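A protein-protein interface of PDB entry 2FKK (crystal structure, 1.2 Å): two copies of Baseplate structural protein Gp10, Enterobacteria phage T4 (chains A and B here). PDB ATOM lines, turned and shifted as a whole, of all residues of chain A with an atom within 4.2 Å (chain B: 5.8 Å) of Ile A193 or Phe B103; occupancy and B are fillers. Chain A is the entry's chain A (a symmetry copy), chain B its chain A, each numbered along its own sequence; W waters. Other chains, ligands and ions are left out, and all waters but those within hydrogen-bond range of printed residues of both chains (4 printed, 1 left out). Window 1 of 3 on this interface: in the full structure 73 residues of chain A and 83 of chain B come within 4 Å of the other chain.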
ATOM      1  N   GLY A  88     -27.344 -33.707 -21.311  1.00  0.00           N
ATOM      2  CA  GLY A  88     -27.145 -32.708 -22.337  1.00  0.00           C
ATOM      3  C   GLY A  88     -27.998 -32.892 -23.561  1.00  0.00           C
ATOM      4  O   GLY A  88     -27.823 -32.137 -24.532  1.00  0.00           O
ATOM      5  N   THR A 127     -25.115 -27.917 -30.564  1.00  0.00           N
ATOM      6  CA  THR A 127     -25.528 -26.794 -29.780  1.00  0.00           C
ATOM      7  C   THR A 127     -25.444 -25.455 -30.522  1.00  0.00           C
ATOM      8  O   THR A 127     -26.119 -24.516 -30.107  1.00  0.00           O
ATOM      9  CB  THR A 127     -24.713 -26.666 -28.487  1.00  0.00           C
ATOM     10  OG1 THR A 127     -23.379 -26.534 -28.878  1.00  0.00           O
ATOM     11  CG2 THR A 127     -24.911 -27.886 -27.575  1.00  0.00           C
ATOM     12  N   THR A 191     -26.655 -19.810 -31.872  1.00  0.00           N
ATOM     13  CA  THR A 191     -27.297 -20.875 -31.106  1.00  0.00           C
ATOM     14  C   THR A 191     -28.119 -21.758 -32.018  1.00  0.00           C
ATOM     15  O   THR A 191     -28.766 -21.283 -32.944  1.00  0.00           O
ATOM     16  CB  THR A 191     -28.142 -20.286 -29.992  1.00  0.00           C
ATOM     17  OG1 THR A 191     -28.581 -21.408 -29.192  1.00  0.00           O
ATOM     18  CG2 THR A 191     -29.371 -19.533 -30.436  1.00  0.00           C
ATOM     19  N   ASN A 192     -28.144 -23.042 -31.639  1.00  0.00           N
ATOM     20  CA  ASN A 192     -29.015 -24.012 -32.251  1.00  0.00           C
ATOM     21  C   ASN A 192     -29.914 -24.658 -31.193  1.00  0.00           C
ATOM     22  O   ASN A 192     -30.410 -25.750 -31.442  1.00  0.00           O
ATOM     23  CB  ASN A 192     -28.227 -25.063 -33.036  1.00  0.00           C
ATOM     24  CG  ASN A 192     -29.089 -25.916 -33.920  1.00  0.00           C
ATOM     25  OD1 ASN A 192     -30.045 -25.481 -34.556  1.00  0.00           O
ATOM     26  ND2 ASN A 192     -28.684 -27.165 -34.012  1.00  0.00           N
ATOM     27  N   ILE A 193     -30.101 -24.042 -30.066  1.00  0.00           N
ATOM     28  CA  ILE A 193     -30.857 -24.625 -28.936  1.00  0.00           C
ATOM     29  C   ILE A 193     -32.180 -23.904 -28.787  1.00  0.00           C
ATOM     30  O   ILE A 193     -32.200 -22.659 -28.674  1.00  0.00           O
ATOM     31  CB  ILE A 193     -30.037 -24.510 -27.633  1.00  0.00           C
ATOM     32  CG1 ILE A 193     -28.693 -25.263 -27.735  1.00  0.00           C
ATOM     33  CG2 ILE A 193     -30.857 -24.965 -26.454  1.00  0.00           C
ATOM     34  CD1 ILE A 193     -27.763 -24.971 -26.576  1.00  0.00           C
ATOM     35  N   GLN A 194     -33.295 -24.631 -28.814  1.00  0.00           N
ATOM     36  CA  GLN A 194     -34.625 -24.081 -28.647  1.00  0.00           C
ATOM     37  C   GLN A 194     -34.933 -23.972 -27.168  1.00  0.00           C
ATOM     38  O   GLN A 194     -34.186 -24.499 -26.326  1.00  0.00           O
ATOM     39  CB  GLN A 194     -35.645 -24.862 -29.439  1.00  0.00           C
ATOM     40  CG  GLN A 194     -36.075 -26.199 -28.816  1.00  0.00           C
ATOM     41  CD  GLN A 194     -37.058 -26.878 -29.714  1.00  0.00           C
ATOM     42  OE1 GLN A 194     -36.715 -27.392 -30.779  1.00  0.00           O
ATOM     43  NE2 GLN A 194     -38.341 -26.863 -29.316  1.00  0.00           N
ATOM     44  N   TYR A 196     -35.554 -24.422 -23.477  1.00  0.00           N
ATOM     45  CA  TYR A 196     -35.404 -25.639 -22.653  1.00  0.00           C
ATOM     46  C   TYR A 196     -35.465 -25.334 -21.194  1.00  0.00           C
ATOM     47  O   TYR A 196     -35.223 -24.224 -20.736  1.00  0.00           O
ATOM     48  CB  TYR A 196     -34.072 -26.358 -22.996  1.00  0.00           C
ATOM     49  CG  TYR A 196     -32.840 -25.625 -22.509  1.00  0.00           C
ATOM     50  CD1 TYR A 196     -32.330 -25.762 -21.208  1.00  0.00           C
ATOM     51  CD2 TYR A 196     -32.167 -24.749 -23.354  1.00  0.00           C
ATOM     52  CE1 TYR A 196     -31.235 -25.070 -20.769  1.00  0.00           C
ATOM     53  CE2 TYR A 196     -31.073 -24.059 -22.932  1.00  0.00           C
ATOM     54  CZ  TYR A 196     -30.605 -24.218 -21.661  1.00  0.00           C
ATOM     55  OH  TYR A 196     -29.512 -23.488 -21.290  1.00  0.00           O
ATOM     56  N   THR A 198     -33.701 -27.881 -17.923  1.00  0.00           N
ATOM     57  CA  THR A 198     -33.055 -29.161 -17.603  1.00  0.00           C
ATOM     58  C   THR A 198     -33.803 -29.851 -16.441  1.00  0.00           C
ATOM     59  O   THR A 198     -34.382 -29.211 -15.583  1.00  0.00           O
ATOM     60  CB  THR A 198     -31.592 -29.034 -17.236  1.00  0.00           C
ATOM     61  OG1 THR A 198     -31.545 -28.325 -15.998  1.00  0.00           O
ATOM     62  CG2 THR A 198     -30.773 -28.291 -18.305  1.00  0.00           C
ATOM     63  N   VAL B  92     -34.202 -31.008 -21.313  1.00  0.00           N
ATOM     64  CA  VAL B  92     -32.844 -31.483 -21.562  1.00  0.00           C
ATOM     65  C   VAL B  92     -32.353 -32.169 -20.326  1.00  0.00           C
ATOM     66  O   VAL B  92     -32.588 -31.733 -19.217  1.00  0.00           O
ATOM     67  CB  VAL B  92     -31.932 -30.336 -22.028  1.00  0.00           C
ATOM     68  CG1 VAL B  92     -30.507 -30.859 -22.235  1.00  0.00           C
ATOM     69  CG2 VAL B  92     -32.445 -29.704 -23.313  1.00  0.00           C
ATOM     70  N   GLY B  93     -31.639 -33.293 -20.520  1.00  0.00           N
ATOM     71  CA  GLY B  93     -31.057 -33.962 -19.367  1.00  0.00           C
ATOM     72  C   GLY B  93     -29.997 -33.127 -18.721  1.00  0.00           C
ATOM     73  O   GLY B  93     -29.041 -32.681 -19.365  1.00  0.00           O
ATOM     74  N   TRP B  94     -30.119 -32.908 -17.416  1.00  0.00           N
ATOM     75  CA  TRP B  94     -29.081 -32.250 -16.661  1.00  0.00           C
ATOM     76  C   TRP B  94     -27.792 -33.033 -16.752  1.00  0.00           C
ATOM     77  O   TRP B  94     -27.802 -34.272 -16.754  1.00  0.00           O
ATOM     78  CB  TRP B  94     -29.506 -32.133 -15.227  1.00  0.00           C
ATOM     79  CG  TRP B  94     -28.514 -31.594 -14.276  1.00  0.00           C
ATOM     80  CD1 TRP B  94     -28.178 -30.298 -14.066  1.00  0.00           C
ATOM     81  CD2 TRP B  94     -27.686 -32.357 -13.386  1.00  0.00           C
ATOM     82  NE1 TRP B  94     -27.219 -30.205 -13.089  1.00  0.00           N
ATOM     83  CE2 TRP B  94     -26.899 -31.472 -12.654  1.00  0.00           C
ATOM     84  CE3 TRP B  94     -27.558 -33.729 -13.186  1.00  0.00           C
ATOM     85  CZ2 TRP B  94     -26.009 -31.906 -11.692  1.00  0.00           C
ATOM     86  CZ3 TRP B  94     -26.671 -34.149 -12.227  1.00  0.00           C
ATOM     87  CH2 TRP B  94     -25.905 -33.233 -11.501  1.00  0.00           C
ATOM     88  N   ASN B  95     -26.689 -32.319 -16.834  1.00  0.00           N
ATOM     89  CA  ASN B  95     -25.399 -32.921 -16.992  1.00  0.00           C
ATOM     90  C   ASN B  95     -24.580 -32.868 -15.707  1.00  0.00           C
ATOM     91  O   ASN B  95     -24.343 -31.758 -15.181  1.00  0.00           O
ATOM     92  CB  ASN B  95     -24.618 -32.262 -18.134  1.00  0.00           C
ATOM     93  CG  ASN B  95     -23.585 -33.144 -18.728  1.00  0.00           C
ATOM     94  OD1 ASN B  95     -23.062 -34.059 -18.094  1.00  0.00           O
ATOM     95  ND2 ASN B  95     -23.256 -32.882 -20.000  1.00  0.00           N
ATOM     96  N   ASP B 100     -20.253 -28.717 -19.091  1.00  0.00           N
ATOM     97  CA  ASP B 100     -21.278 -28.496 -20.118  1.00  0.00           C
ATOM     98  C   ASP B 100     -21.698 -27.037 -20.055  1.00  0.00           C
ATOM     99  O   ASP B 100     -22.172 -26.587 -18.995  1.00  0.00           O
ATOM    100  CB  ASP B 100     -22.465 -29.406 -19.842  1.00  0.00           C
ATOM    101  CG  ASP B 100     -23.561 -29.366 -20.906  1.00  0.00           C
ATOM    102  OD1 ASP B 100     -23.829 -28.288 -21.451  1.00  0.00           O
ATOM    103  OD2 ASP B 100     -24.163 -30.429 -21.193  1.00  0.00           O
ATOM    104  N   PRO B 101     -21.595 -26.251 -21.109  1.00  0.00           N
ATOM    105  CA  PRO B 101     -21.856 -24.816 -21.010  1.00  0.00           C
ATOM    106  C   PRO B 101     -23.325 -24.438 -21.021  1.00  0.00           C
ATOM    107  O   PRO B 101     -23.668 -23.254 -20.841  1.00  0.00           O
ATOM    108  CB  PRO B 101     -21.127 -24.213 -22.215  1.00  0.00           C
ATOM    109  CG  PRO B 101     -21.094 -25.330 -23.162  1.00  0.00           C
ATOM    110  CD  PRO B 101     -21.016 -26.615 -22.415  1.00  0.00           C
ATOM    111  N   ASN B 102     -24.186 -25.411 -21.247  1.00  0.00           N
ATOM    112  CA  ASN B 102     -25.621 -25.146 -21.328  1.00  0.00           C
ATOM    113  C   ASN B 102     -26.427 -25.877 -20.259  1.00  0.00           C
ATOM    114  O   ASN B 102     -27.428 -25.317 -19.824  1.00  0.00           O
ATOM    115  CB  ASN B 102     -26.180 -25.583 -22.704  1.00  0.00           C
ATOM    116  CG  ASN B 102     -25.464 -24.855 -23.809  1.00  0.00           C
ATOM    117  OD1 ASN B 102     -25.604 -23.632 -23.919  1.00  0.00           O
ATOM    118  ND2 ASN B 102     -24.701 -25.578 -24.593  1.00  0.00           N
ATOM    119  N   PHE B 103     -26.073 -27.124 -19.954  1.00  0.00           N
ATOM    120  CA  PHE B 103     -27.017 -28.029 -19.310  1.00  0.00           C
ATOM    121  C   PHE B 103     -26.570 -28.567 -17.948  1.00  0.00           C
ATOM    122  O   PHE B 103     -27.183 -29.480 -17.427  1.00  0.00           O
ATOM    123  CB  PHE B 103     -27.345 -29.174 -20.270  1.00  0.00           C
ATOM    124  CG  PHE B 103     -27.868 -28.670 -21.594  1.00  0.00           C
ATOM    125  CD1 PHE B 103     -28.931 -27.812 -21.692  1.00  0.00           C
ATOM    126  CD2 PHE B 103     -27.269 -29.082 -22.771  1.00  0.00           C
ATOM    127  CE1 PHE B 103     -29.432 -27.394 -22.911  1.00  0.00           C
ATOM    128  CE2 PHE B 103     -27.749 -28.679 -24.018  1.00  0.00           C
ATOM    129  CZ  PHE B 103     -28.825 -27.821 -24.101  1.00  0.00           C
ATOM    130  N   ALA B 104     -25.531 -27.974 -17.378  1.00  0.00           N
ATOM    131  CA  ALA B 104     -25.065 -28.294 -16.054  1.00  0.00           C
ATOM    132  C   ALA B 104     -25.412 -27.273 -14.992  1.00  0.00           C
ATOM    133  O   ALA B 104     -25.794 -27.627 -13.860  1.00  0.00           O
ATOM    134  CB  ALA B 104     -23.542 -28.498 -16.042  1.00  0.00           C
ATOM    135  N   LEU B 105     -25.228 -25.992 -15.286  1.00  0.00           N
ATOM    136  CA  LEU B 105     -25.281 -24.950 -14.288  1.00  0.00           C
ATOM    137  C   LEU B 105     -26.553 -24.133 -14.399  1.00  0.00           C
ATOM    138  O   LEU B 105     -26.967 -23.762 -15.484  1.00  0.00           O
ATOM    139  CB  LEU B 105     -24.056 -24.044 -14.415  1.00  0.00           C
ATOM    140  CG  LEU B 105     -22.706 -24.755 -14.257  1.00  0.00           C
ATOM    141  CD1 LEU B 105     -21.535 -23.754 -14.451  1.00  0.00           C
ATOM    142  CD2 LEU B 105     -22.618 -25.466 -12.953  1.00  0.00           C
ATOM    143  N   THR B 119     -27.214 -27.689 -10.509  1.00  0.00           N
ATOM    144  CA  THR B 119     -28.513 -28.283 -10.298  1.00  0.00           C
ATOM    145  C   THR B 119     -29.303 -28.229 -11.594  1.00  0.00           C
ATOM    146  O   THR B 119     -29.045 -27.398 -12.460  1.00  0.00           O
ATOM    147  CB  THR B 119     -29.343 -27.538  -9.201  1.00  0.00           C
ATOM    148  OG1 THR B 119     -29.532 -26.189  -9.616  1.00  0.00           O
ATOM    149  CG2 THR B 119     -28.675 -27.627  -7.829  1.00  0.00           C
ATOM    150  N   GLY B 124     -32.844 -21.773 -20.998  1.00  0.00           N
ATOM    151  CA  GLY B 124     -32.231 -21.022 -22.070  1.00  0.00           C
ATOM    152  C   GLY B 124     -32.874 -21.380 -23.375  1.00  0.00           C
ATOM    153  O   GLY B 124     -33.942 -21.968 -23.411  1.00  0.00           O
ATOM    154  N   GLY B 125     -32.193 -21.042 -24.470  1.00  0.00           N
ATOM    155  CA  GLY B 125     -32.663 -21.319 -25.793  1.00  0.00           C
ATOM    156  C   GLY B 125     -33.573 -20.269 -26.347  1.00  0.00           C
ATOM    157  O   GLY B 125     -34.055 -19.388 -25.650  1.00  0.00           O
ATOM    158  N   SER B 126     -33.787 -20.382 -27.681  1.00  0.00           N
ATOM    159  CA  SER B 126     -34.502 -19.362 -28.412  1.00  0.00           C
ATOM    160  C   SER B 126     -35.353 -19.986 -29.508  1.00  0.00           C
ATOM    161  O   SER B 126     -34.935 -20.964 -30.126  1.00  0.00           O
ATOM    162  CB  SER B 126     -33.429 -18.420 -29.112  1.00  0.00           C
ATOM    163  OG  SER B 126     -32.725 -17.712 -28.148  1.00  0.00           O
ATOM    164  N   THR B 127     -36.536 -19.416 -29.779  1.00  0.00           N
ATOM    165  CA  THR B 127     -37.386 -19.916 -30.814  1.00  0.00           C
ATOM    166  C   THR B 127     -36.933 -19.533 -32.228  1.00  0.00           C
ATOM    167  O   THR B 127     -37.337 -20.208 -33.171  1.00  0.00           O
ATOM    168  CB  THR B 127     -38.836 -19.448 -30.642  1.00  0.00           C
ATOM    169  OG1 THR B 127     -38.800 -18.051 -30.662  1.00  0.00           O
ATOM    170  CG2 THR B 127     -39.446 -19.974 -29.334  1.00  0.00           C
ATOM    171  N   ASN B 192     -35.657 -21.645 -35.103  1.00  0.00           N
ATOM    172  CA  ASN B 192     -34.694 -22.413 -34.354  1.00  0.00           C
ATOM    173  C   ASN B 192     -35.379 -23.602 -33.676  1.00  0.00           C
ATOM    174  O   ASN B 192     -34.832 -24.110 -32.705  1.00  0.00           O
ATOM    175  CB  ASN B 192     -33.944 -21.543 -33.341  1.00  0.00           C
ATOM    176  CG  ASN B 192     -32.746 -22.223 -32.748  1.00  0.00           C
ATOM    177  OD1 ASN B 192     -31.989 -22.946 -33.391  1.00  0.00           O
ATOM    178  ND2 ASN B 192     -32.533 -21.917 -31.486  1.00  0.00           N
HETATM  179  O   HOH W   1     -27.632 -22.235 -22.857  1.00  0.00           O
HETATM  180  O   HOH W   2     -29.156 -22.964 -18.623  1.00  0.00           O
HETATM  181  O   HOH W   3     -23.017 -24.212 -26.615  1.00  0.00           O
HETATM  182  O   HOH W   4     -29.465 -26.862 -15.156  1.00  0.00           O
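The backbone carbonyl oxygen (O) of Gly B93 is in hydrogen-bond range of the backbone NH (N) of Gly A88 (2.8 Å).
The side-chain hydroxyl of Tyr A196 sits at hydrogen-bond distance from the backbone carbonyl oxygen of Asn B102 (3.1 Å).
The backbone NH (N) of Tyr A196 is in hydrogen-bond range of the backbone carbonyl oxygen (O) of Gly B124 (2.9 Å).
The backbone NH of Ser B126 lies within hydrogen-bond range of the backbone carbonyl oxygen of Ile A193.
The side-chain amide oxygen (OD1) of Asn A192 sits close to the side-chain amide oxygen (OD1) of Asn B192, at 3.4 Å.
The side-chain amide nitrogen (ND2) of Asn B192 is in hydrogen-bond range of the backbone carbonyl oxygen (O) of Ile A193, 2.9 Å away.
The side-chain amide nitrogen (ND2) of Asn B95 sits at hydrogen-bond distance from the side-chain carboxylate (OD2) of Asp B100 (2.9 Å).
O of Phe B103 sits at hydrogen-bond distance from N of Asn B95, 2.9 Å away.
N of Asn B102 is in hydrogen-bond range of OD1 of Asp B100 (2.9 Å).
The side-chain carboxylate (OD1) of Asp B100 is in hydrogen-bond range of the backbone NH (N) of Phe B103, 2.9 Å away.
N of Asn B192 sits at hydrogen-bond distance from O of Thr B127.
The side-chain hydroxyl (OG1) of Thr A191 lies within hydrogen-bond range of the backbone NH (N) of Ile A193 (3.2 Å).
Val B92 touches Gly A88.
OD2 of Asp B100 touches CA of Gly A88 (3.9 Å).
Phe B103 touches Gly A88.
Asn B192 touches Thr A191 (OD1 to O, 3.7 Å).
Ile A193 touches Phe B103 (CD1 to CZ, 3.9 Å).
O of Gly B124 touches O of Gln A194, 3.9 Å away.
O of Asn B192 touches CB of Gln A194, 3.4 Å away.
Gly B125 touches Tyr A196 (N to CE2, 3.6 Å).
Val B92 touches Thr A198.
Phe B103 touches Thr A198.
Printed residues of chain B within 4 Å of Gly A88: Val B92, Gly B93, Asp B100 and Phe B103.
Printed residues of chain B within 4 Å of Thr A191: Asn B192 (3.7 Å).
Ile A193 touches just these residues of chain B: Asn B102, Phe B103, Gly B125, Ser B126 and Asn B192.
Printed residues of chain A within 4 Å of Gly B93: Gly A88 (2.8 Å).
Of the printed residues of chain A, Asp B100 touches Gly A88.
Phe B103 touches just these residues of chain A: Gly A88, Ile A193, Tyr A196 and Thr A198.
The nearest printed residue of chain B that does not touch Thr A191 is Ser B126 (4.4 Å).
Of the 8 printed residues of chain A, 8 touch a printed residue of chain B.
Printed residues of chain A that touch a printed residue of chain B: Gly A88, Thr A127, Thr A191, Asn A192, Ile A193, Gln A194, Tyr A196 and Thr A198.
Hydrophobic or aromatic side chains of chain B within 4 Å of the printed part of chain A: Val B92 and Phe B103.
Among the printed residues, 23 pairs touch across the chains.
Among the printed residues, no Asp or Glu carboxylate lies within 4 Å of a Lys or Arg side-chain nitrogen of the other chain.
Asn A192 touches its own counterpart, Asn B192.
Of the 23 pairs that touch across the chains among the printed residues, 1 has its exchanged pair printed and touching as well.
Water W4 lies within hydrogen-bond range of OG1 of Thr A198 (2.7 Å) and O of Thr B119 (2.8 Å).
Water W1 bridges the side-chain amide oxygen of Asn B102 and the side-chain hydroxyl of Tyr A196.
Water W2 lies within hydrogen-bond range of the side-chain hydroxyl (OH) of Tyr A196 (2.7 Å) and the backbone carbonyl oxygen (O) of Asn B102 (3.2 Å).
Water W3 bridges the side-chain amide nitrogen (ND2) of Asn B102 (3.0 Å) and the side-chain hydroxyl (OG1) of Thr A127 (3.3 Å).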
